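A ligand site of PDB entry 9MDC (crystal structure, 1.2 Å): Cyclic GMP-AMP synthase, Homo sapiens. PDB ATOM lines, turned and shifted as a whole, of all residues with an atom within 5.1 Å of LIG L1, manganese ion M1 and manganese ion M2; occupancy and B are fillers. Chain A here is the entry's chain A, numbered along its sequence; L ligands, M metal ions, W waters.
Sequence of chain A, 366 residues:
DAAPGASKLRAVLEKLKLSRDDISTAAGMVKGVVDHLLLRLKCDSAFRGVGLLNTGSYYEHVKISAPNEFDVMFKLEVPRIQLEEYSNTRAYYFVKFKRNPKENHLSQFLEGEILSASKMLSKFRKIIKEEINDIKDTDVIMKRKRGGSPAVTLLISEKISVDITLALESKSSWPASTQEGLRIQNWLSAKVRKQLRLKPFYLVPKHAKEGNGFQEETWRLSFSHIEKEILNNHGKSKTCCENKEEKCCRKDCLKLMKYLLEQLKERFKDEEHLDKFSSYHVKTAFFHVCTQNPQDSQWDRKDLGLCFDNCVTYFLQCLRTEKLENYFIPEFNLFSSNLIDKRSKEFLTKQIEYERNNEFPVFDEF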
ATOM      1  N   THR A  55      28.974  -5.523 -12.405  1.00  0.00           N
ATOM      2  CA  THR A  55      28.536  -5.532 -13.799  1.00  0.00           C
ATOM      3  C   THR A  55      27.161  -4.901 -13.900  1.00  0.00           C
ATOM      4  O   THR A  55      26.537  -4.556 -12.892  1.00  0.00           O
ATOM      5  CB  THR A  55      28.443  -6.971 -14.348  1.00  0.00           C
ATOM      6  OG1 THR A  55      27.454  -7.708 -13.617  1.00  0.00           O
ATOM      7  CG2 THR A  55      29.784  -7.705 -14.253  1.00  0.00           C
ATOM      8  N   GLY A  56      26.655  -4.794 -15.144  1.00  0.00           N
ATOM      9  CA  GLY A  56      25.300  -4.348 -15.355  1.00  0.00           C
ATOM     10  C   GLY A  56      25.114  -2.851 -15.209  1.00  0.00           C
ATOM     11  O   GLY A  56      26.061  -2.065 -15.015  1.00  0.00           O
ATOM     12  N   SER A  57      23.841  -2.440 -15.276  1.00  0.00           N
ATOM     13  CA  SER A  57      23.547  -1.041 -15.590  1.00  0.00           C
ATOM     14  C   SER A  57      23.973  -0.073 -14.497  1.00  0.00           C
ATOM     15  O   SER A  57      24.298   1.073 -14.799  1.00  0.00           O
ATOM     16  CB  SER A  57      22.068  -0.845 -15.898  1.00  0.00           C
ATOM     17  OG  SER A  57      21.276  -1.123 -14.754  1.00  0.00           O
ATOM     18  N   GLU A  60      27.513   0.635 -15.113  1.00  0.00           N
ATOM     19  CA  GLU A  60      27.645   1.270 -16.418  1.00  0.00           C
ATOM     20  C   GLU A  60      27.001   2.648 -16.455  1.00  0.00           C
ATOM     21  O   GLU A  60      27.007   3.297 -17.506  1.00  0.00           O
ATOM     22  CB  GLU A  60      27.015   0.358 -17.491  1.00  0.00           C
ATOM     23  CG  GLU A  60      27.756  -0.963 -17.677  1.00  0.00           C
ATOM     24  CD  GLU A  60      26.942  -2.046 -18.358  1.00  0.00           C
ATOM     25  OE1 GLU A  60      27.544  -3.002 -18.888  1.00  0.00           O
ATOM     26  OE2 GLU A  60      25.697  -1.906 -18.414  1.00  0.00           O
ATOM     27  N   VAL A  62      23.923   3.495 -16.459  1.00  0.00           N
ATOM     28  CA  VAL A  62      22.707   3.556 -17.277  1.00  0.00           C
ATOM     29  C   VAL A  62      21.518   2.939 -16.533  1.00  0.00           C
ATOM     30  O   VAL A  62      20.481   2.640 -17.148  1.00  0.00           O
ATOM     31  CB  VAL A  62      22.898   2.976 -18.693  1.00  0.00           C
ATOM     32  CG1 VAL A  62      23.921   3.810 -19.506  1.00  0.00           C
ATOM     33  CG2 VAL A  62      23.304   1.500 -18.635  1.00  0.00           C
ATOM     34  N   LYS A  63      21.631   2.767 -15.218  1.00  0.00           N
ATOM     35  CA  LYS A  63      20.471   2.396 -14.414  1.00  0.00           C
ATOM     36  C   LYS A  63      19.504   3.567 -14.368  1.00  0.00           C
ATOM     37  O   LYS A  63      19.918   4.711 -14.172  1.00  0.00           O
ATOM     38  CB  LYS A  63      20.924   2.019 -13.005  1.00  0.00           C
ATOM     39  CG  LYS A  63      19.805   1.614 -12.069  1.00  0.00           C
ATOM     40  CD  LYS A  63      19.391   0.173 -12.319  1.00  0.00           C
ATOM     41  CE  LYS A  63      18.141  -0.237 -11.531  1.00  0.00           C
ATOM     42  NZ  LYS A  63      16.904   0.449 -12.037  1.00  0.00           N
ATOM     43  N   GLU A  69      18.394  -2.292  -8.429  1.00  0.00           N
ATOM     44  CA  GLU A  69      18.771  -3.570  -9.026  1.00  0.00           C
ATOM     45  C   GLU A  69      20.248  -3.520  -9.395  1.00  0.00           C
ATOM     46  O   GLU A  69      20.672  -2.655 -10.179  1.00  0.00           O
ATOM     47  CB  GLU A  69      17.894  -3.945 -10.223  1.00  0.00           C
ATOM     48  CG  GLU A  69      17.855  -5.460 -10.519  1.00  0.00           C
ATOM     49  CD  GLU A  69      18.894  -5.921 -11.497  1.00  0.00           C
ATOM     50  OE1 GLU A  69      19.670  -5.096 -12.022  1.00  0.00           O
ATOM     51  OE2 GLU A  69      18.893  -7.140 -11.775  1.00  0.00           O
ATOM     52  N   PHE A  70      21.017  -4.426  -8.798  1.00  0.00           N
ATOM     53  CA  PHE A  70      22.463  -4.478  -8.932  1.00  0.00           C
ATOM     54  C   PHE A  70      22.858  -5.862  -9.419  1.00  0.00           C
ATOM     55  O   PHE A  70      22.247  -6.866  -9.053  1.00  0.00           O
ATOM     56  CB  PHE A  70      23.156  -4.282  -7.577  1.00  0.00           C
ATOM     57  CG  PHE A  70      23.022  -2.892  -7.003  1.00  0.00           C
ATOM     58  CD1 PHE A  70      21.829  -2.466  -6.437  1.00  0.00           C
ATOM     59  CD2 PHE A  70      24.096  -2.010  -7.018  1.00  0.00           C
ATOM     60  CE1 PHE A  70      21.709  -1.190  -5.905  1.00  0.00           C
ATOM     61  CE2 PHE A  70      23.985  -0.746  -6.456  1.00  0.00           C
ATOM     62  CZ  PHE A  70      22.787  -0.335  -5.905  1.00  0.00           C
ATOM     63  N   ASP A  71      23.952  -5.918 -10.184  1.00  0.00           N
ATOM     64  CA  ASP A  71      24.475  -7.172 -10.714  1.00  0.00           C
ATOM     65  C   ASP A  71      25.940  -7.305 -10.358  1.00  0.00           C
ATOM     66  O   ASP A  71      26.738  -6.390 -10.567  1.00  0.00           O
ATOM     67  CB  ASP A  71      24.315  -7.219 -12.225  1.00  0.00           C
ATOM     68  CG  ASP A  71      22.903  -6.961 -12.640  1.00  0.00           C
ATOM     69  OD1 ASP A  71      22.097  -7.909 -12.514  1.00  0.00           O
ATOM     70  OD2 ASP A  71      22.603  -5.833 -13.086  1.00  0.00           O
ATOM     71  N   ASP A 163      21.606  -9.473  -8.095  1.00  0.00           N
ATOM     72  CA  ASP A 163      21.912 -10.727  -8.790  1.00  0.00           C
ATOM     73  C   ASP A 163      23.381 -11.069  -8.580  1.00  0.00           C
ATOM     74  O   ASP A 163      24.248 -10.298  -8.972  1.00  0.00           O
ATOM     75  CB  ASP A 163      21.615 -10.581 -10.285  1.00  0.00           C
ATOM     76  CG  ASP A 163      20.136 -10.475 -10.600  1.00  0.00           C
ATOM     77  OD1 ASP A 163      19.324 -10.929  -9.760  1.00  0.00           O
ATOM     78  OD2 ASP A 163      19.798  -9.947 -11.668  1.00  0.00           O
ATOM     79  N   ARG A 220      27.853 -21.113 -19.887  1.00  0.00           N
ATOM     80  CA  ARG A 220      27.692 -20.160 -20.970  1.00  0.00           C
ATOM     81  C   ARG A 220      28.743 -19.055 -20.878  1.00  0.00           C
ATOM     82  O   ARG A 220      29.074 -18.572 -19.782  1.00  0.00           O
ATOM     83  CB  ARG A 220      26.303 -19.528 -20.950  1.00  0.00           C
ATOM     84  CG  ARG A 220      26.063 -18.589 -22.108  1.00  0.00           C
ATOM     85  CD  ARG A 220      24.612 -18.359 -22.342  1.00  0.00           C
ATOM     86  NE  ARG A 220      24.374 -17.239 -23.244  1.00  0.00           N
ATOM     87  CZ  ARG A 220      23.178 -16.895 -23.698  1.00  0.00           C
ATOM     88  NH1 ARG A 220      22.112 -17.638 -23.449  1.00  0.00           N
ATOM     89  NH2 ARG A 220      23.046 -15.768 -24.389  1.00  0.00           N
ATOM     90  N   SER A 224      30.383  -9.754 -19.783  1.00  0.00           N
ATOM     91  CA  SER A 224      29.736  -8.608 -19.155  1.00  0.00           C
ATOM     92  C   SER A 224      30.742  -7.553 -18.714  1.00  0.00           C
ATOM     93  O   SER A 224      30.425  -6.352 -18.683  1.00  0.00           O
ATOM     94  CB  SER A 224      28.885  -9.086 -17.971  1.00  0.00           C
ATOM     95  OG  SER A 224      28.110  -8.033 -17.436  1.00  0.00           O
ATOM     96  N   GLU A 227      31.469  -5.440 -21.817  1.00  0.00           N
ATOM     97  CA  GLU A 227      30.367  -4.512 -22.032  1.00  0.00           C
ATOM     98  C   GLU A 227      30.494  -3.294 -21.145  1.00  0.00           C
ATOM     99  O   GLU A 227      30.264  -2.155 -21.597  1.00  0.00           O
ATOM    100  CB  GLU A 227      29.041  -5.225 -21.780  1.00  0.00           C
ATOM    101  CG  GLU A 227      28.848  -6.397 -22.710  1.00  0.00           C
ATOM    102  CD  GLU A 227      27.649  -7.268 -22.364  1.00  0.00           C
ATOM    103  OE1 GLU A 227      26.867  -6.927 -21.442  1.00  0.00           O
ATOM    104  OE2 GLU A 227      27.481  -8.307 -23.025  1.00  0.00           O
ATOM    105  N   LYS A 258      15.766   1.523 -23.095  1.00  0.00           N
ATOM    106  CA  LYS A 258      15.416   0.639 -21.984  1.00  0.00           C
ATOM    107  C   LYS A 258      14.066   1.015 -21.381  1.00  0.00           C
ATOM    108  O   LYS A 258      13.267   0.144 -21.041  1.00  0.00           O
ATOM    109  CB  LYS A 258      16.500   0.666 -20.920  1.00  0.00           C
ATOM    110  CG  LYS A 258      16.161  -0.240 -19.744  1.00  0.00           C
ATOM    111  CD  LYS A 258      17.403  -0.594 -18.955  1.00  0.00           C
ATOM    112  CE  LYS A 258      18.153   0.645 -18.512  1.00  0.00           C
ATOM    113  NZ  LYS A 258      19.407   0.268 -17.804  1.00  0.00           N
ATOM    114  N   SER A 279      16.140  -6.172 -21.245  1.00  0.00           N
ATOM    115  CA  SER A 279      17.011  -5.034 -21.505  1.00  0.00           C
ATOM    116  C   SER A 279      18.270  -5.455 -22.259  1.00  0.00           C
ATOM    117  O   SER A 279      18.861  -4.617 -22.949  1.00  0.00           O
ATOM    118  CB  SER A 279      17.313  -4.256 -20.233  1.00  0.00           C
ATOM    119  OG  SER A 279      18.146  -5.027 -19.434  1.00  0.00           O
ATOM    120  N   TYR A 280      18.670  -6.737 -22.199  1.00  0.00           N
ATOM    121  CA  TYR A 280      19.852  -7.155 -22.959  1.00  0.00           C
ATOM    122  C   TYR A 280      19.608  -7.097 -24.452  1.00  0.00           C
ATOM    123  O   TYR A 280      20.547  -6.887 -25.236  1.00  0.00           O
ATOM    124  CB  TYR A 280      20.299  -8.564 -22.557  1.00  0.00           C
ATOM    125  CG  TYR A 280      21.702  -8.853 -23.038  1.00  0.00           C
ATOM    126  CD1 TYR A 280      22.793  -8.188 -22.493  1.00  0.00           C
ATOM    127  CD2 TYR A 280      21.958  -9.775 -24.047  1.00  0.00           C
ATOM    128  CE1 TYR A 280      24.081  -8.424 -22.921  1.00  0.00           C
ATOM    129  CE2 TYR A 280      23.246 -10.021 -24.485  1.00  0.00           C
ATOM    130  CZ  TYR A 280      24.303  -9.351 -23.917  1.00  0.00           C
ATOM    131  OH  TYR A 280      25.562  -9.605 -24.368  1.00  0.00           O
ATOM    132  N   LYS A 283      20.284  -3.526 -25.153  1.00  0.00           N
ATOM    133  CA  LYS A 283      21.716  -3.283 -24.990  1.00  0.00           C
ATOM    134  C   LYS A 283      22.494  -3.787 -26.193  1.00  0.00           C
ATOM    135  O   LYS A 283      23.379  -3.102 -26.724  1.00  0.00           O
ATOM    136  CB  LYS A 283      22.195  -3.959 -23.697  1.00  0.00           C
ATOM    137  CG  LYS A 283      23.578  -3.528 -23.231  1.00  0.00           C
ATOM    138  CD  LYS A 283      24.074  -4.382 -22.054  1.00  0.00           C
ATOM    139  CE  LYS A 283      25.256  -3.713 -21.342  1.00  0.00           C
ATOM    140  NZ  LYS A 283      25.839  -4.585 -20.278  1.00  0.00           N
ATOM    141  N   ASN A 326      24.347 -11.702 -31.152  1.00  0.00           N
ATOM    142  CA  ASN A 326      25.127 -11.393 -29.967  1.00  0.00           C
ATOM    143  C   ASN A 326      26.369 -10.608 -30.367  1.00  0.00           C
ATOM    144  O   ASN A 326      26.991 -10.874 -31.396  1.00  0.00           O
ATOM    145  CB  ASN A 326      25.487 -12.701 -29.262  1.00  0.00           C
ATOM    146  CG  ASN A 326      26.287 -12.487 -27.986  1.00  0.00           C
ATOM    147  OD1 ASN A 326      27.484 -12.270 -28.041  1.00  0.00           O
ATOM    148  ND2 ASN A 326      25.607 -12.564 -26.842  1.00  0.00           N
HETATM  149  P1  LIG L   1      18.773  -3.127 -15.993  1.00  0.00           P
HETATM  150  O1  LIG L   1      17.458  -3.511 -16.665  1.00  0.00           O
HETATM  151  O2  LIG L   1      19.128  -3.962 -14.791  1.00  0.00           O
HETATM  152  O3  LIG L   1      18.898  -1.632 -15.780  1.00  0.00           O
HETATM  153  P2  LIG L   1      21.201  -4.540 -17.006  1.00  0.00           P
HETATM  154  O4  LIG L   1      22.068  -4.475 -18.209  1.00  0.00           O
HETATM  155  O5  LIG L   1      21.824  -4.465 -15.644  1.00  0.00           O
HETATM  156  N1  LIG L   1      20.008  -3.444 -17.192  1.00  0.00           N
HETATM  157  P3  LIG L   1      20.276  -7.273 -16.229  1.00  0.00           P
HETATM  158  O6  LIG L   1      19.118  -8.025 -16.776  1.00  0.00           O
HETATM  159  O7  LIG L   1      20.282  -6.919 -14.753  1.00  0.00           O
HETATM  160  O8  LIG L   1      20.413  -5.990 -17.129  1.00  0.00           O
HETATM  161  O9  LIG L   1      21.590  -8.105 -16.601  1.00  0.00           O
HETATM  162  C1  LIG L   1      22.834  -7.788 -16.005  1.00  0.00           C
HETATM  163  C2  LIG L   1      23.948  -8.085 -16.991  1.00  0.00           C
HETATM  164  O10 LIG L   1      23.966  -9.503 -17.284  1.00  0.00           O
HETATM  165  C3  LIG L   1      23.819  -7.456 -18.383  1.00  0.00           C
HETATM  166  O11 LIG L   1      24.196  -6.110 -18.416  1.00  0.00           O
HETATM  167  C4  LIG L   1      24.639  -8.401 -19.233  1.00  0.00           C
HETATM  168  O12 LIG L   1      26.005  -8.033 -19.133  1.00  0.00           O
HETATM  169  C5  LIG L   1      24.354  -9.782 -18.580  1.00  0.00           C
HETATM  170  N2  LIG L   1      23.265 -10.449 -19.272  1.00  0.00           N
HETATM  171  C6  LIG L   1      21.913 -10.389 -19.031  1.00  0.00           C
HETATM  172  N3  LIG L   1      21.199 -11.075 -19.881  1.00  0.00           N
HETATM  173  C7  LIG L   1      22.121 -11.619 -20.737  1.00  0.00           C
HETATM  174  C8  LIG L   1      22.017 -12.454 -21.869  1.00  0.00           C
HETATM  175  N4  LIG L   1      20.838 -12.901 -22.343  1.00  0.00           N
HETATM  176  N5  LIG L   1      23.135 -12.791 -22.504  1.00  0.00           N
HETATM  177  C9  LIG L   1      24.305 -12.353 -22.051  1.00  0.00           C
HETATM  178  N6  LIG L   1      24.526 -11.577 -21.013  1.00  0.00           N
HETATM  179  C10 LIG L   1      23.404 -11.233 -20.384  1.00  0.00           C
HETATM  180  C1  LG2 L   2      25.134 -13.761 -18.059  1.00  0.00           C
HETATM  181  C2  LG2 L   2      19.031 -12.930 -15.722  1.00  0.00           C
HETATM  182  C3  LG2 L   2      21.423 -12.222 -15.546  1.00  0.00           C
HETATM  183  C4  LG2 L   2      19.703 -10.655 -14.931  1.00  0.00           C
HETATM  184  C5  LG2 L   2      18.304 -10.073 -14.916  1.00  0.00           C
HETATM  185  C6  LG2 L   2      16.874  -8.540 -14.002  1.00  0.00           C
HETATM  186  C7  LG2 L   2      15.868  -8.938 -14.858  1.00  0.00           C
HETATM  187  C8  LG2 L   2      16.190  -9.928 -15.769  1.00  0.00           C
HETATM  188  C9  LG2 L   2      14.438  -7.061 -14.285  1.00  0.00           C
HETATM  189  C10 LG2 L   2      13.007  -6.671 -14.507  1.00  0.00           C
HETATM  190  C11 LG2 L   2      21.939 -12.840 -14.254  1.00  0.00           C
HETATM  191  C12 LG2 L   2      24.756 -14.501 -19.170  1.00  0.00           C
HETATM  192  C13 LG2 L   2      23.412 -14.763 -19.398  1.00  0.00           C
HETATM  193  C14 LG2 L   2      22.454 -14.246 -18.539  1.00  0.00           C
HETATM  194  C15 LG2 L   2      22.838 -13.470 -17.422  1.00  0.00           C
HETATM  195  C16 LG2 L   2      24.198 -13.233 -17.182  1.00  0.00           C
HETATM  196  C17 LG2 L   2      20.597 -13.613 -17.472  1.00  0.00           C
HETATM  197  C18 LG2 L   2      21.625 -13.088 -16.753  1.00  0.00           C
HETATM  198  C19 LG2 L   2      19.143 -13.428 -17.165  1.00  0.00           C
HETATM  199  N1  LG2 L   2      21.082 -14.324 -18.543  1.00  0.00           N
HETATM  200  N2  LG2 L   2      19.996 -11.881 -15.427  1.00  0.00           N
HETATM  201  N3  LG2 L   2      18.080  -9.105 -14.029  1.00  0.00           N
HETATM  202  N4  LG2 L   2      17.400 -10.488 -15.809  1.00  0.00           N
HETATM  203  O1  LG2 L   2      20.566  -9.925 -14.439  1.00  0.00           O
HETATM  204  O2  LG2 L   2      14.619  -8.365 -14.848  1.00  0.00           O
HETATM  205  O3  LG2 L   2      12.131  -7.656 -13.988  1.00  0.00           O
HETATM  206 CL1  LG2 L   2      25.976 -15.107 -20.260  1.00  0.00          CL
HETATM  207 CL2  LG2 L   2      22.876 -15.680 -20.762  1.00  0.00          CL
HETATM  208 MN    MN M   1      20.073  -8.348 -13.041  1.00  0.00          MN
HETATM  209 MN    MN M   2      20.758  -4.943 -13.842  1.00  0.00          MN
HETATM  210  O   HOH W   1      23.058  -2.083 -19.073  1.00  0.00           O
HETATM  211  O   HOH W   2      18.673  -8.085 -19.506  1.00  0.00           O
HETATM  212  O   HOH W   3      21.026  -6.167 -20.276  1.00  0.00           O
HETATM  213  O   HOH W   4      17.269   0.414 -14.931  1.00  0.00           O
HETATM  214  O   HOH W   5      16.797  -6.227 -16.687  1.00  0.00           O
HETATM  215  O   HOH W   6      17.803 -11.927 -22.911  1.00  0.00           O
HETATM  216  O   HOH W   7      16.754  -4.975 -13.708  1.00  0.00           O
HETATM  217  O   HOH W   8      23.071 -13.270 -25.487  1.00  0.00           O
HETATM  218  O   HOH W   9      21.536  -3.059 -12.880  1.00  0.00           O
HETATM  219  O   HOH W  10      27.206 -11.342 -20.292  1.00  0.00           O
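An oxygen (O5) of LIG L1 lies close to the backbone NH (N) of Ser 57, at 2.9 Å.
The side-chain hydroxyl (OG) of Ser 57 lies within hydrogen-bond range of an oxygen (O3) of LIG L1 (2.6 Å).
An oxygen (O12) of LIG L1 sits at hydrogen-bond distance from the side-chain carboxylate of Glu 227 (2.7 Å).
The side-chain hydroxyl of Ser 224 lies within hydrogen-bond range of an oxygen (O12) of LIG L1, at 2.7 Å.
The side-chain amino group of Lys 258 is in salt-bridge range of an oxygen (O3) of LIG L1 (2.8 Å).
O11 of LIG L1 sits at hydrogen-bond distance from NZ of Lys 283.
An oxygen (O1) of LIG L1 lies within hydrogen-bond range of the side-chain hydroxyl (OG) of Ser 279, 3.2 Å away.
The backbone NH (N) of Asp 163 lies within hydrogen-bond range of the backbone carbonyl oxygen (O) of Phe 70 (2.9 Å).
The backbone carbonyl oxygen (O) of Asp 71 lies within hydrogen-bond range of the backbone NH (N) of Thr 55.
The backbone carbonyl oxygen (O) of Ser 57 sits at hydrogen-bond distance from the backbone NH (N) of Lys 63, at 3.2 Å.
The backbone NH (N) of Val 62 sits at hydrogen-bond distance from the backbone carbonyl oxygen (O) of Ser 57.
The side-chain amino group (NZ) of Lys 283 is in salt-bridge range of the side-chain carboxylate (OE1) of Glu 227, 2.8 Å away.
The side-chain carboxylate (OE2) of Glu 227 sits at hydrogen-bond distance from the side-chain hydroxyl (OH) of Tyr 280.
NZ of Lys 258 is in hydrogen-bond range of O of Val 62 (2.7 Å).
The side-chain carboxylate of Glu 60 is in salt-bridge range of the side-chain amino group of Lys 283 (2.7 Å).
Merely in contact with LIG L1: Gly 56 (3.5 Å), Lys 63 (3.9 Å), Arg 220 (3.5 Å) and Tyr 280 (3.4 Å).
Hydrophobic or aromatic side chains within 4 Å of LIG L1: Tyr 280.
12 residues have an atom within 4 Å of LIG L1: Gly 56, Ser 57, Lys 63, Glu 69, Asp 71, Arg 220, Ser 224, Glu 227, Lys 258, Ser 279, Tyr 280 and Lys 283.
Of the 18 residues printed, 3 come within 4 Å of manganese ion M1.
Ser 57 touches manganese ion M2 (OG to MN, 3.96 Å).
Three residues have an atom within 4 Å of manganese ion M2: Ser 57, Glu 69 and Asp 71.
Manganese ion M1 is bound by OE2 of Glu 69, OD2 of Asp 163, OD1 of Asp 71, O1 of LG2 L2, O7 of LIG L1 and N3 of LG2 L2.
The side-chain carboxylate (OE1) of Glu 69 is bound to manganese ion M2, at 2.1 Å.
O2 of LIG L1 binds manganese ion M2, 2.1 Å away.
O5 of LIG L1 binds manganese ion M2.
The side-chain carboxylate (OD2) of Asp 71 binds manganese ion M2 (2.2 Å).
Manganese ion M2 is bound by O7 of LIG L1 (2.2 Å).
Manganese ion M2 is bound by water W9 (2.3 Å).
Manganese ion M2 has six donor atoms within binding distance.
Water W9 bridges the side-chain hydroxyl of Ser 57 (2.7 Å) and the backbone carbonyl oxygen of Glu 69 (2.9 Å).
Water W1 bridges OE2 of Glu 60 and O4 of LIG L1.
Water W2 lies within hydrogen-bond range of O6 of LIG L1 (2.8 Å), N of Tyr 280 (3.0 Å) and OG of Ser 279 (3.1 Å).
Water W5 bridges O1 of LIG L1 (2.8 Å) and OG of Ser 279 (3.3 Å).
Water W3 lies within hydrogen-bond range of O4 of LIG L1 (2.9 Å), N of Tyr 280 (3.1 Å) and OG of Ser 279 (3.2 Å).
Water W8 lies within hydrogen-bond range of the guanidinium group (NH2) of Arg 220 (2.7 Å), the side-chain amide nitrogen (ND2) of Asn 326 (3.0 Å) and a nitrogen (N5) of LIG L1 (3.0 Å).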
